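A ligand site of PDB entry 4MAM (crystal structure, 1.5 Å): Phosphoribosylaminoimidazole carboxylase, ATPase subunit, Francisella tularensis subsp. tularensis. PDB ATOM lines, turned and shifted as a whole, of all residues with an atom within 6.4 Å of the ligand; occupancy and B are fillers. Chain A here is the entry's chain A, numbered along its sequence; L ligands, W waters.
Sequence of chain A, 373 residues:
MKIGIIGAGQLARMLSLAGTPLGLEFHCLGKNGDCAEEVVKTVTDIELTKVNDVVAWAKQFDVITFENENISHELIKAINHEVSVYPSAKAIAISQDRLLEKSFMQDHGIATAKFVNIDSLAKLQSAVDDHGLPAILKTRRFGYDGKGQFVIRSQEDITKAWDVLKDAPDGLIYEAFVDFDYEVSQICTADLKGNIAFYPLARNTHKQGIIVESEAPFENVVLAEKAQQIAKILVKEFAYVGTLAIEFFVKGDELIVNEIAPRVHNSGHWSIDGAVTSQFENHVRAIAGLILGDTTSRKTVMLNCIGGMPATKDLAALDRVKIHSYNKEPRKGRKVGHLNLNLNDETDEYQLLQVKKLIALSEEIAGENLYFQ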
ATOM      1  N   ARG A  98      15.153   6.901  -2.540  1.00  0.00           N
ATOM      2  CA  ARG A  98      16.049   7.487  -3.530  1.00  0.00           C
ATOM      3  C   ARG A  98      15.354   8.469  -4.462  1.00  0.00           C
ATOM      4  O   ARG A  98      15.937   9.463  -4.860  1.00  0.00           O
ATOM      5  CB  ARG A  98      16.732   6.403  -4.372  1.00  0.00           C
ATOM      6  CG  ARG A  98      17.568   5.429  -3.559  1.00  0.00           C
ATOM      7  CD  ARG A  98      18.414   4.564  -4.519  1.00  0.00           C
ATOM      8  NE  ARG A  98      19.135   3.518  -3.803  1.00  0.00           N
ATOM      9  CZ  ARG A  98      20.254   3.733  -3.102  1.00  0.00           C
ATOM     10  NH1 ARG A  98      20.845   2.727  -2.458  1.00  0.00           N
ATOM     11  NH2 ARG A  98      20.772   4.949  -3.038  1.00  0.00           N
ATOM     12  N   LYS A 102      16.387  12.379  -4.624  1.00  0.00           N
ATOM     13  CA  LYS A 102      16.815  13.002  -5.873  1.00  0.00           C
ATOM     14  C   LYS A 102      15.912  14.150  -6.263  1.00  0.00           C
ATOM     15  O   LYS A 102      16.375  15.189  -6.740  1.00  0.00           O
ATOM     16  CB  LYS A 102      16.816  11.969  -7.003  1.00  0.00           C
ATOM     17  CG  LYS A 102      17.886  10.892  -6.904  1.00  0.00           C
ATOM     18  CD  LYS A 102      19.132  11.286  -7.663  1.00  0.00           C
ATOM     19  CE  LYS A 102      20.066  10.090  -7.834  1.00  0.00           C
ATOM     20  NZ  LYS A 102      20.659   9.607  -6.541  1.00  0.00           N
ATOM     21  N   ALA A 113      22.871  12.675 -10.150  1.00  0.00           N
ATOM     22  CA  ALA A 113      22.782  11.826 -11.329  1.00  0.00           C
ATOM     23  C   ALA A 113      21.452  12.080 -12.028  1.00  0.00           C
ATOM     24  O   ALA A 113      20.462  12.452 -11.394  1.00  0.00           O
ATOM     25  CB  ALA A 113      22.886  10.358 -10.941  1.00  0.00           C
ATOM     26  N   LYS A 114      21.412  11.886 -13.340  1.00  0.00           N
ATOM     27  CA  LYS A 114      20.138  11.858 -14.032  1.00  0.00           C
ATOM     28  C   LYS A 114      19.396  10.615 -13.544  1.00  0.00           C
ATOM     29  O   LYS A 114      19.985   9.546 -13.400  1.00  0.00           O
ATOM     30  CB  LYS A 114      20.327  11.826 -15.549  1.00  0.00           C
ATOM     31  CG  LYS A 114      20.585  13.202 -16.141  1.00  0.00           C
ATOM     32  CD  LYS A 114      21.059  13.110 -17.585  1.00  0.00           C
ATOM     33  CE  LYS A 114      22.545  12.835 -17.647  1.00  0.00           C
ATOM     34  N   ILE A 136      22.572   2.418 -13.666  1.00  0.00           N
ATOM     35  CA  ILE A 136      22.337   1.544 -12.528  1.00  0.00           C
ATOM     36  C   ILE A 136      20.853   1.555 -12.211  1.00  0.00           C
ATOM     37  O   ILE A 136      20.232   2.615 -12.200  1.00  0.00           O
ATOM     38  CB  ILE A 136      23.094   2.012 -11.262  1.00  0.00           C
ATOM     39  CG1 ILE A 136      24.563   2.307 -11.617  1.00  0.00           C
ATOM     40  CG2 ILE A 136      23.007   0.960 -10.173  1.00  0.00           C
ATOM     41  CD1 ILE A 136      25.331   3.030 -10.521  1.00  0.00           C
ATOM     42  N   LYS A 138      18.316   0.761  -9.147  1.00  0.00           N
ATOM     43  CA  LYS A 138      18.438   0.690  -7.681  1.00  0.00           C
ATOM     44  C   LYS A 138      17.078   0.627  -7.039  1.00  0.00           C
ATOM     45  O   LYS A 138      16.143   1.277  -7.495  1.00  0.00           O
ATOM     46  CB  LYS A 138      19.144   1.954  -7.156  1.00  0.00           C
ATOM     47  CG  LYS A 138      20.490   2.262  -7.768  1.00  0.00           C
ATOM     48  CD  LYS A 138      21.119   3.442  -7.028  1.00  0.00           C
ATOM     49  CE  LYS A 138      22.463   3.831  -7.619  1.00  0.00           C
ATOM     50  NZ  LYS A 138      23.009   5.055  -6.924  1.00  0.00           N
ATOM     51  N   GLY A 143      18.117  -0.017   0.410  1.00  0.00           N
ATOM     52  CA  GLY A 143      19.460  -0.244  -0.083  1.00  0.00           C
ATOM     53  C   GLY A 143      20.544   0.244   0.867  1.00  0.00           C
ATOM     54  O   GLY A 143      20.460   1.331   1.445  1.00  0.00           O
ATOM     55  N   TYR A 144      21.584  -0.564   1.033  1.00  0.00           N
ATOM     56  CA  TYR A 144      22.765  -0.157   1.782  1.00  0.00           C
ATOM     57  C   TYR A 144      23.942  -1.011   1.333  1.00  0.00           C
ATOM     58  O   TYR A 144      23.751  -2.146   0.862  1.00  0.00           O
ATOM     59  CB  TYR A 144      22.537  -0.292   3.299  1.00  0.00           C
ATOM     60  CG  TYR A 144      22.397  -1.722   3.772  1.00  0.00           C
ATOM     61  CD1 TYR A 144      21.170  -2.367   3.702  1.00  0.00           C
ATOM     62  CD2 TYR A 144      23.484  -2.408   4.279  1.00  0.00           C
ATOM     63  CE1 TYR A 144      21.038  -3.677   4.127  1.00  0.00           C
ATOM     64  CE2 TYR A 144      23.363  -3.717   4.704  1.00  0.00           C
ATOM     65  CZ  TYR A 144      22.134  -4.347   4.630  1.00  0.00           C
ATOM     66  OH  TYR A 144      22.000  -5.640   5.064  1.00  0.00           O
ATOM     67  N   ASP A 145      25.146  -0.467   1.474  1.00  0.00           N
ATOM     68  CA  ASP A 145      26.380  -1.167   1.075  1.00  0.00           C
ATOM     69  C   ASP A 145      26.276  -1.740  -0.342  1.00  0.00           C
ATOM     70  O   ASP A 145      26.783  -2.830  -0.631  1.00  0.00           O
ATOM     71  CB  ASP A 145      26.742  -2.272   2.084  1.00  0.00           C
ATOM     72  CG  ASP A 145      27.074  -1.712   3.451  1.00  0.00           C
ATOM     73  OD1 ASP A 145      27.337  -0.499   3.545  1.00  0.00           O
ATOM     74  OD2 ASP A 145      27.104  -2.498   4.424  1.00  0.00           O
ATOM     75  N   GLY A 146      25.595  -0.996  -1.210  1.00  0.00           N
ATOM     76  CA  GLY A 146      25.477  -1.388  -2.607  1.00  0.00           C
ATOM     77  C   GLY A 146      24.420  -2.427  -2.912  1.00  0.00           C
ATOM     78  O   GLY A 146      24.251  -2.818  -4.072  1.00  0.00           O
ATOM     79  N   LYS A 147      23.698  -2.897  -1.891  1.00  0.00           N
ATOM     80  CA  LYS A 147      22.683  -3.929  -2.089  1.00  0.00           C
ATOM     81  C   LYS A 147      21.437  -3.380  -2.798  1.00  0.00           C
ATOM     82  O   LYS A 147      21.136  -2.191  -2.690  1.00  0.00           O
ATOM     83  CB  LYS A 147      22.278  -4.547  -0.757  1.00  0.00           C
ATOM     84  CG  LYS A 147      23.421  -5.307  -0.074  1.00  0.00           C
ATOM     85  CD  LYS A 147      22.981  -5.759   1.302  1.00  0.00           C
ATOM     86  CE  LYS A 147      24.119  -6.436   2.042  1.00  0.00           C
ATOM     87  NZ  LYS A 147      23.629  -7.053   3.305  1.00  0.00           N
ATOM     88  N   GLN A 149      20.990  -3.305  -6.097  1.00  0.00           N
ATOM     89  CA  GLN A 149      21.390  -2.574  -7.299  1.00  0.00           C
ATOM     90  C   GLN A 149      21.804  -3.527  -8.404  1.00  0.00           C
ATOM     91  O   GLN A 149      22.259  -4.644  -8.151  1.00  0.00           O
ATOM     92  CB  GLN A 149      22.549  -1.611  -7.012  1.00  0.00           C
ATOM     93  CG  GLN A 149      22.242  -0.640  -5.885  1.00  0.00           C
ATOM     94  CD  GLN A 149      23.172   0.539  -5.858  1.00  0.00           C
ATOM     95  OE1 GLN A 149      23.924   0.799  -6.800  1.00  0.00           O
ATOM     96  NE2 GLN A 149      23.129   1.283  -4.760  1.00  0.00           N
ATOM     97  N   GLU A 175      19.457   5.305 -12.593  1.00  0.00           N
ATOM     98  CA  GLU A 175      20.418   6.399 -12.567  1.00  0.00           C
ATOM     99  C   GLU A 175      21.364   6.243 -13.743  1.00  0.00           C
ATOM    100  O   GLU A 175      21.859   5.155 -14.020  1.00  0.00           O
ATOM    101  CB  GLU A 175      21.234   6.396 -11.283  1.00  0.00           C
ATOM    102  CG  GLU A 175      20.463   6.707 -10.020  1.00  0.00           C
ATOM    103  CD  GLU A 175      21.369   6.845  -8.818  1.00  0.00           C
ATOM    104  OE1 GLU A 175      22.593   7.045  -9.012  1.00  0.00           O
ATOM    105  OE2 GLU A 175      20.861   6.765  -7.684  1.00  0.00           O
ATOM    106  N   ALA A 176      21.624   7.352 -14.435  1.00  0.00           N
ATOM    107  CA  ALA A 176      22.703   7.361 -15.406  1.00  0.00           C
ATOM    108  C   ALA A 176      24.028   7.368 -14.680  1.00  0.00           C
ATOM    109  O   ALA A 176      24.151   7.926 -13.589  1.00  0.00           O
ATOM    110  CB  ALA A 176      22.585   8.562 -16.325  1.00  0.00           C
ATOM    111  N   PHE A 177      25.028   6.733 -15.273  1.00  0.00           N
ATOM    112  CA  PHE A 177      26.355   6.735 -14.686  1.00  0.00           C
ATOM    113  C   PHE A 177      26.912   8.137 -14.657  1.00  0.00           C
ATOM    114  O   PHE A 177      26.939   8.819 -15.674  1.00  0.00           O
ATOM    115  CB  PHE A 177      27.302   5.852 -15.495  1.00  0.00           C
ATOM    116  CG  PHE A 177      27.841   4.700 -14.725  1.00  0.00           C
ATOM    117  CD1 PHE A 177      27.025   3.612 -14.439  1.00  0.00           C
ATOM    118  CD2 PHE A 177      29.166   4.680 -14.332  1.00  0.00           C
ATOM    119  CE1 PHE A 177      27.532   2.522 -13.750  1.00  0.00           C
ATOM    120  CE2 PHE A 177      29.671   3.594 -13.629  1.00  0.00           C
ATOM    121  CZ  PHE A 177      28.854   2.514 -13.339  1.00  0.00           C
ATOM    122  N   VAL A 178      27.358   8.568 -13.484  1.00  0.00           N
ATOM    123  CA  VAL A 178      27.971   9.871 -13.360  1.00  0.00           C
ATOM    124  C   VAL A 178      29.448   9.770 -13.703  1.00  0.00           C
ATOM    125  O   VAL A 178      30.146   8.842 -13.253  1.00  0.00           O
ATOM    126  CB  VAL A 178      27.813  10.433 -11.941  1.00  0.00           C
ATOM    127  CG1 VAL A 178      28.552  11.775 -11.806  1.00  0.00           C
ATOM    128  CG2 VAL A 178      26.349  10.609 -11.625  1.00  0.00           C
ATOM    129  N   ASP A 179      29.912  10.705 -14.520  1.00  0.00           N
ATOM    130  CA  ASP A 179      31.323  10.918 -14.785  1.00  0.00           C
ATOM    131  C   ASP A 179      31.929  11.667 -13.596  1.00  0.00           C
ATOM    132  O   ASP A 179      31.660  12.858 -13.396  1.00  0.00           O
ATOM    133  CB  ASP A 179      31.485  11.742 -16.065  1.00  0.00           C
ATOM    134  CG  ASP A 179      32.924  12.077 -16.376  1.00  0.00           C
ATOM    135  OD1 ASP A 179      33.834  11.509 -15.740  1.00  0.00           O
ATOM    136  OD2 ASP A 179      33.138  12.897 -17.294  1.00  0.00           O
ATOM    137  N   PHE A 180      32.729  10.972 -12.780  1.00  0.00           N
ATOM    138  CA  PHE A 180      33.384  11.606 -11.641  1.00  0.00           C
ATOM    139  C   PHE A 180      34.806  11.099 -11.421  1.00  0.00           C
ATOM    140  O   PHE A 180      35.164  10.016 -11.879  1.00  0.00           O
ATOM    141  CB  PHE A 180      32.542  11.511 -10.350  1.00  0.00           C
ATOM    142  CG  PHE A 180      32.373  10.111  -9.815  1.00  0.00           C
ATOM    143  CD1 PHE A 180      33.354   9.521  -9.030  1.00  0.00           C
ATOM    144  CD2 PHE A 180      31.209   9.404 -10.066  1.00  0.00           C
ATOM    145  CE1 PHE A 180      33.192   8.241  -8.521  1.00  0.00           C
ATOM    146  CE2 PHE A 180      31.027   8.121  -9.559  1.00  0.00           C
ATOM    147  CZ  PHE A 180      32.029   7.538  -8.781  1.00  0.00           C
ATOM    148  N   GLU A 183      35.245  10.455  -4.800  1.00  0.00           N
ATOM    149  CA  GLU A 183      34.083  10.696  -3.955  1.00  0.00           C
ATOM    150  C   GLU A 183      34.504  11.304  -2.629  1.00  0.00           C
ATOM    151  O   GLU A 183      35.555  10.946  -2.059  1.00  0.00           O
ATOM    152  CB  GLU A 183      33.321   9.386  -3.732  1.00  0.00           C
ATOM    153  CG  GLU A 183      32.776   8.779  -5.014  1.00  0.00           C
ATOM    154  CD  GLU A 183      32.043   7.468  -4.779  1.00  0.00           C
ATOM    155  OE1 GLU A 183      32.575   6.412  -5.187  1.00  0.00           O
ATOM    156  OE2 GLU A 183      30.940   7.494  -4.199  1.00  0.00           O
ATOM    157  N   HIS A 206      35.548   3.253  -2.380  1.00  0.00           N
ATOM    158  CA  HIS A 206      34.619   2.127  -2.378  1.00  0.00           C
ATOM    159  C   HIS A 206      35.147   0.973  -3.203  1.00  0.00           C
ATOM    160  O   HIS A 206      35.908   1.175  -4.164  1.00  0.00           O
ATOM    161  CB  HIS A 206      33.241   2.568  -2.908  1.00  0.00           C
ATOM    162  CG  HIS A 206      32.638   3.718  -2.143  1.00  0.00           C
ATOM    163  ND1 HIS A 206      33.033   5.033  -2.345  1.00  0.00           N
ATOM    164  CD2 HIS A 206      31.694   3.758  -1.177  1.00  0.00           C
ATOM    165  CE1 HIS A 206      32.350   5.819  -1.528  1.00  0.00           C
ATOM    166  NE2 HIS A 206      31.537   5.076  -0.816  1.00  0.00           N
ATOM    167  N   GLY A 209      30.860  -1.390  -4.360  1.00  0.00           N
ATOM    168  CA  GLY A 209      29.706  -0.735  -3.769  1.00  0.00           C
ATOM    169  C   GLY A 209      29.715  -0.501  -2.264  1.00  0.00           C
ATOM    170  O   GLY A 209      28.752   0.040  -1.721  1.00  0.00           O
ATOM    171  N   ILE A 210      30.783  -0.901  -1.591  1.00  0.00           N
ATOM    172  CA  ILE A 210      30.893  -0.710  -0.144  1.00  0.00           C
ATOM    173  C   ILE A 210      32.100   0.163   0.176  1.00  0.00           C
ATOM    174  O   ILE A 210      33.149   0.051  -0.474  1.00  0.00           O
ATOM    175  CB  ILE A 210      30.941  -2.061   0.626  1.00  0.00           C
ATOM    176  CG1 ILE A 210      30.678  -1.840   2.131  1.00  0.00           C
ATOM    177  CG2 ILE A 210      32.261  -2.769   0.418  1.00  0.00           C
ATOM    178  CD1 ILE A 210      30.405  -3.133   2.904  1.00  0.00           C
ATOM    179  N   GLU A 247      26.915  12.443   0.828  1.00  0.00           N
ATOM    180  CA  GLU A 247      27.879  11.808  -0.074  1.00  0.00           C
ATOM    181  C   GLU A 247      27.869  12.513  -1.421  1.00  0.00           C
ATOM    182  O   GLU A 247      26.806  12.729  -1.989  1.00  0.00           O
ATOM    183  CB  GLU A 247      27.508  10.341  -0.306  1.00  0.00           C
ATOM    184  CG  GLU A 247      27.661   9.460   0.924  1.00  0.00           C
ATOM    185  CD  GLU A 247      27.194   8.040   0.681  1.00  0.00           C
ATOM    186  OE1 GLU A 247      27.154   7.594  -0.483  1.00  0.00           O
ATOM    187  OE2 GLU A 247      26.866   7.351   1.680  1.00  0.00           O
ATOM    188  N   PHE A 249      29.766  12.940  -5.478  1.00  0.00           N
ATOM    189  CA  PHE A 249      30.702  12.636  -6.553  1.00  0.00           C
ATOM    190  C   PHE A 249      31.412  13.951  -6.888  1.00  0.00           C
ATOM    191  O   PHE A 249      30.774  15.001  -6.906  1.00  0.00           O
ATOM    192  CB  PHE A 249      29.956  12.146  -7.796  1.00  0.00           C
ATOM    193  CG  PHE A 249      29.125  10.909  -7.580  1.00  0.00           C
ATOM    194  CD1 PHE A 249      29.616   9.838  -6.847  1.00  0.00           C
ATOM    195  CD2 PHE A 249      27.844  10.830  -8.117  1.00  0.00           C
ATOM    196  CE1 PHE A 249      28.837   8.690  -6.672  1.00  0.00           C
ATOM    197  CE2 PHE A 249      27.064   9.696  -7.947  1.00  0.00           C
ATOM    198  CZ  PHE A 249      27.556   8.621  -7.227  1.00  0.00           C
ATOM    199  N   ASN A 258      25.346  12.396  -4.385  1.00  0.00           N
ATOM    200  CA  ASN A 258      25.002  10.984  -4.542  1.00  0.00           C
ATOM    201  C   ASN A 258      23.779  10.666  -3.683  1.00  0.00           C
ATOM    202  O   ASN A 258      22.709  10.353  -4.209  1.00  0.00           O
ATOM    203  CB  ASN A 258      26.190  10.125  -4.128  1.00  0.00           C
ATOM    204  CG  ASN A 258      25.888   8.644  -4.186  1.00  0.00           C
ATOM    205  OD1 ASN A 258      25.069   8.209  -5.002  1.00  0.00           O
ATOM    206  ND2 ASN A 258      26.543   7.865  -3.326  1.00  0.00           N
ATOM    207  N   GLU A 259      23.936  10.807  -2.364  1.00  0.00           N
ATOM    208  CA  GLU A 259      22.808  10.586  -1.463  1.00  0.00           C
ATOM    209  C   GLU A 259      23.118  11.166  -0.098  1.00  0.00           C
ATOM    210  O   GLU A 259      24.259  11.563   0.167  1.00  0.00           O
ATOM    211  CB  GLU A 259      22.474   9.092  -1.358  1.00  0.00           C
ATOM    212  CG  GLU A 259      23.549   8.248  -0.710  1.00  0.00           C
ATOM    213  CD  GLU A 259      23.161   6.787  -0.620  1.00  0.00           C
ATOM    214  OE1 GLU A 259      21.973   6.458  -0.792  1.00  0.00           O
ATOM    215  OE2 GLU A 259      24.073   5.983  -0.374  1.00  0.00           O
ATOM    216  N   HIS A 265      27.638   8.424  10.080  1.00  0.00           N
ATOM    217  CA  HIS A 265      27.873   7.700   8.836  1.00  0.00           C
ATOM    218  C   HIS A 265      29.258   7.063   8.838  1.00  0.00           C
ATOM    219  O   HIS A 265      30.201   7.610   9.443  1.00  0.00           O
ATOM    220  CB  HIS A 265      27.757   8.714   7.690  1.00  0.00           C
ATOM    221  CG  HIS A 265      27.794   8.122   6.310  1.00  0.00           C
ATOM    222  ND1 HIS A 265      28.950   8.012   5.583  1.00  0.00           N
ATOM    223  CD2 HIS A 265      26.791   7.699   5.498  1.00  0.00           C
ATOM    224  CE1 HIS A 265      28.677   7.510   4.384  1.00  0.00           C
ATOM    225  NE2 HIS A 265      27.373   7.316   4.308  1.00  0.00           N
ATOM    226  N   TYR A 371      31.559  -1.018 -10.500  1.00  0.00           N
ATOM    227  CA  TYR A 371      31.199   0.357 -10.839  1.00  0.00           C
ATOM    228  C   TYR A 371      32.296   1.115 -11.573  1.00  0.00           C
ATOM    229  O   TYR A 371      32.282   2.359 -11.603  1.00  0.00           O
ATOM    230  CB  TYR A 371      30.834   1.135  -9.567  1.00  0.00           C
ATOM    231  CG  TYR A 371      29.610   0.596  -8.851  1.00  0.00           C
ATOM    232  CD1 TYR A 371      29.720  -0.405  -7.902  1.00  0.00           C
ATOM    233  CD2 TYR A 371      28.355   1.109  -9.135  1.00  0.00           C
ATOM    234  CE1 TYR A 371      28.605  -0.884  -7.244  1.00  0.00           C
ATOM    235  CE2 TYR A 371      27.239   0.635  -8.485  1.00  0.00           C
ATOM    236  CZ  TYR A 371      27.367  -0.355  -7.530  1.00  0.00           C
ATOM    237  OH  TYR A 371      26.252  -0.824  -6.889  1.00  0.00           O
ATOM    238  N   GLN A 373      34.564   3.117 -14.087  1.00  0.00           N
ATOM    239  CA  GLN A 373      34.308   4.070 -15.166  1.00  0.00           C
ATOM    240  C   GLN A 373      35.612   4.603 -15.736  1.00  0.00           C
ATOM    241  O   GLN A 373      36.447   3.831 -16.213  1.00  0.00           O
ATOM    242  CB  GLN A 373      33.396   5.211 -14.694  1.00  0.00           C
ATOM    243  CG  GLN A 373      33.953   6.054 -13.546  1.00  0.00           C
ATOM    244  CD  GLN A 373      33.088   7.260 -13.244  1.00  0.00           C
ATOM    245  OE1 GLN A 373      33.279   8.342 -13.803  1.00  0.00           O
ATOM    246  NE2 GLN A 373      32.107   7.090 -12.370  1.00  0.00           N
HETATM  247  P1  LIG L   1      24.463   2.681  -0.991  1.00  0.00           P
HETATM  248  O1  LIG L   1      25.634   3.197  -0.171  1.00  0.00           O
HETATM  249  O2  LIG L   1      23.296   3.615  -0.919  1.00  0.00           O
HETATM  250  O3  LIG L   1      24.083   1.266  -0.706  1.00  0.00           O
HETATM  251  P2  LIG L   1      25.244   4.010  -3.582  1.00  0.00           P
HETATM  252  O4  LIG L   1      23.967   4.348  -4.314  1.00  0.00           O
HETATM  253  O5  LIG L   1      25.790   5.153  -2.760  1.00  0.00           O
HETATM  254  C1  LIG L   1      25.025   2.516  -2.655  1.00  0.00           C
HETATM  255  O6  LIG L   1      26.318   3.451  -4.589  1.00  0.00           O
HETATM  256  C2  LIG L   1      27.509   2.939  -4.009  1.00  0.00           C
HETATM  257  C3  LIG L   1      28.636   3.370  -4.853  1.00  0.00           C
HETATM  258  O7  LIG L   1      28.341   2.948  -6.270  1.00  0.00           O
HETATM  259  C4  LIG L   1      28.800   4.833  -4.932  1.00  0.00           C
HETATM  260  O8  LIG L   1      29.574   5.306  -3.755  1.00  0.00           O
HETATM  261  C5  LIG L   1      29.476   5.019  -6.188  1.00  0.00           C
HETATM  262  O9  LIG L   1      30.873   4.619  -6.069  1.00  0.00           O
HETATM  263  C6  LIG L   1      28.792   4.081  -7.116  1.00  0.00           C
HETATM  264  N1  LIG L   1      27.692   4.687  -7.712  1.00  0.00           N
HETATM  265  C7  LIG L   1      26.401   4.826  -7.232  1.00  0.00           C
HETATM  266  N2  LIG L   1      25.648   5.502  -8.104  1.00  0.00           N
HETATM  267  C8  LIG L   1      26.422   5.840  -9.185  1.00  0.00           C
HETATM  268  C9  LIG L   1      26.181   6.505 -10.363  1.00  0.00           C
HETATM  269  N3  LIG L   1      24.884   7.027 -10.654  1.00  0.00           N
HETATM  270  N4  LIG L   1      27.163   6.666 -11.242  1.00  0.00           N
HETATM  271  C10 LIG L   1      28.409   6.171 -10.994  1.00  0.00           C
HETATM  272  N5  LIG L   1      28.683   5.511  -9.858  1.00  0.00           N
HETATM  273  C11 LIG L   1      27.722   5.325  -8.947  1.00  0.00           C
HETATM  274  O   HOH W   1      22.114   0.237  -2.235  1.00  0.00           O
HETATM  275  O   HOH W   2      27.984   1.991  -0.193  1.00  0.00           O
HETATM  276  O   HOH W   3      31.419   4.489 -10.309  1.00  0.00           O
HETATM  277  O   HOH W   4      25.246   2.323   2.342  1.00  0.00           O
HETATM  278  O   HOH W   5      21.199   3.982   0.903  1.00  0.00           O
HETATM  279  O   HOH W   6      22.796   6.872  -4.187  1.00  0.00           O
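Water W2 bridges the backbone carbonyl oxygen (O) of Gly 209 (2.6 Å) and an oxygen (O1) of the ligand (2.6 Å).
Water W4 lies within hydrogen-bond range of O1 of the ligand (2.7 Å) and N of Asp 145 (2.9 Å).
Water W6 lies within hydrogen-bond range of OD1 of Asn 258, O4 of the ligand, NH2 of Arg 98 and NZ of Lys 138.
Water W5 lies within hydrogen-bond range of an oxygen (O2) of the ligand (2.8 Å), the backbone carbonyl oxygen of Gly 143 (2.8 Å) and the side-chain carboxylate of Glu 259 (3.1 Å).
Water W3 lies within hydrogen-bond range of the backbone carbonyl oxygen (O) of Tyr 371, a nitrogen (N5) of the ligand and the side-chain amide nitrogen (NE2) of Gln 373.
CB of Ala 113 touches N3 of the ligand, at 3.9 Å.
Ile 136 touches the ligand (CD1 to C8, 3.3 Å).
Tyr 144 touches the ligand.
Phe 177 touches the ligand (CA to N4, 3.5 Å).
Phe 180 touches the ligand.
His 206 touches the ligand (NE2 to O8, 3.5 Å).
Gly 209 touches the ligand.
Glu 247 touches the ligand.
Phe 249 touches the ligand (CZ to C8, 3.6 Å).
Tyr 371 touches the ligand (CE2 to O7, 3.4 Å).
Hydrophobic or aromatic side chains that line the ligand: Ala 113, Ile 136, Phe 177, Val 178, Phe 180, His 206, Phe 249 and Tyr 371.
Of the 29 residues printed, 21 come within 4 Å of the ligand.
The nearest printed residue that does not touch the ligand is Gly 143 (4.01 Å).
The side-chain carboxylate of Glu 259 lies close to an oxygen (O2) of the ligand.
An oxygen (O8) of the ligand sits at hydrogen-bond distance from the side-chain carboxylate (OE2) of Glu 183 (2.6 Å).
The backbone NH (N) of Gly 146 is in hydrogen-bond range of an oxygen (O3) of the ligand.
The side-chain carboxylate of Glu 175 lies within hydrogen-bond range of a nitrogen (N3) of the ligand, at 2.8 Å.
The side-chain amino group (NZ) of Lys 138 is in salt-bridge range of an oxygen (O4) of the ligand (2.9 Å).
The side-chain amide nitrogen of Asn 258 is in hydrogen-bond range of an oxygen (O5) of the ligand (2.9 Å).
The backbone NH (N) of Val 178 is in hydrogen-bond range of a nitrogen (N4) of the ligand, 2.9 Å away.
The backbone NH (N) of Asp 145 is in hydrogen-bond range of an oxygen (O3) of the ligand.
NH1 of Arg 98 lies within salt-bridge range of O2 of the ligand, at 3.0 Å.
An oxygen (O4) of the ligand sits close to the side-chain amide nitrogen (NE2) of Gln 149 (3.2 Å).
O of Ala 176 lies within hydrogen-bond range of N3 of the ligand.
A ring nitrogen (ND1) of His 206 lies within hydrogen-bond range of the side-chain carboxylate (OE1) of Glu 183 (3.2 Å).
The side-chain carboxylate (OE2) of Glu 175 lies within salt-bridge range of the side-chain amino group (NZ) of Lys 138 (2.8 Å).
The backbone NH of Glu 175 sits at hydrogen-bond distance from the backbone carbonyl oxygen of Ile 136 (2.8 Å).
The side-chain amino group of Lys 102 lies within salt-bridge range of the side-chain carboxylate of Glu 175 (3.1 Å).
The backbone carbonyl oxygen of Asn 258 lies within hydrogen-bond range of the side-chain amino group of Lys 102.
O of Val 178 sits at hydrogen-bond distance from NE2 of Gln 373 (2.8 Å).
NZ of Lys 147 is in hydrogen-bond range of OH of Tyr 144 (2.8 Å).
OH of Tyr 371 is in hydrogen-bond range of OE1 of Gln 149, 2.8 Å away.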
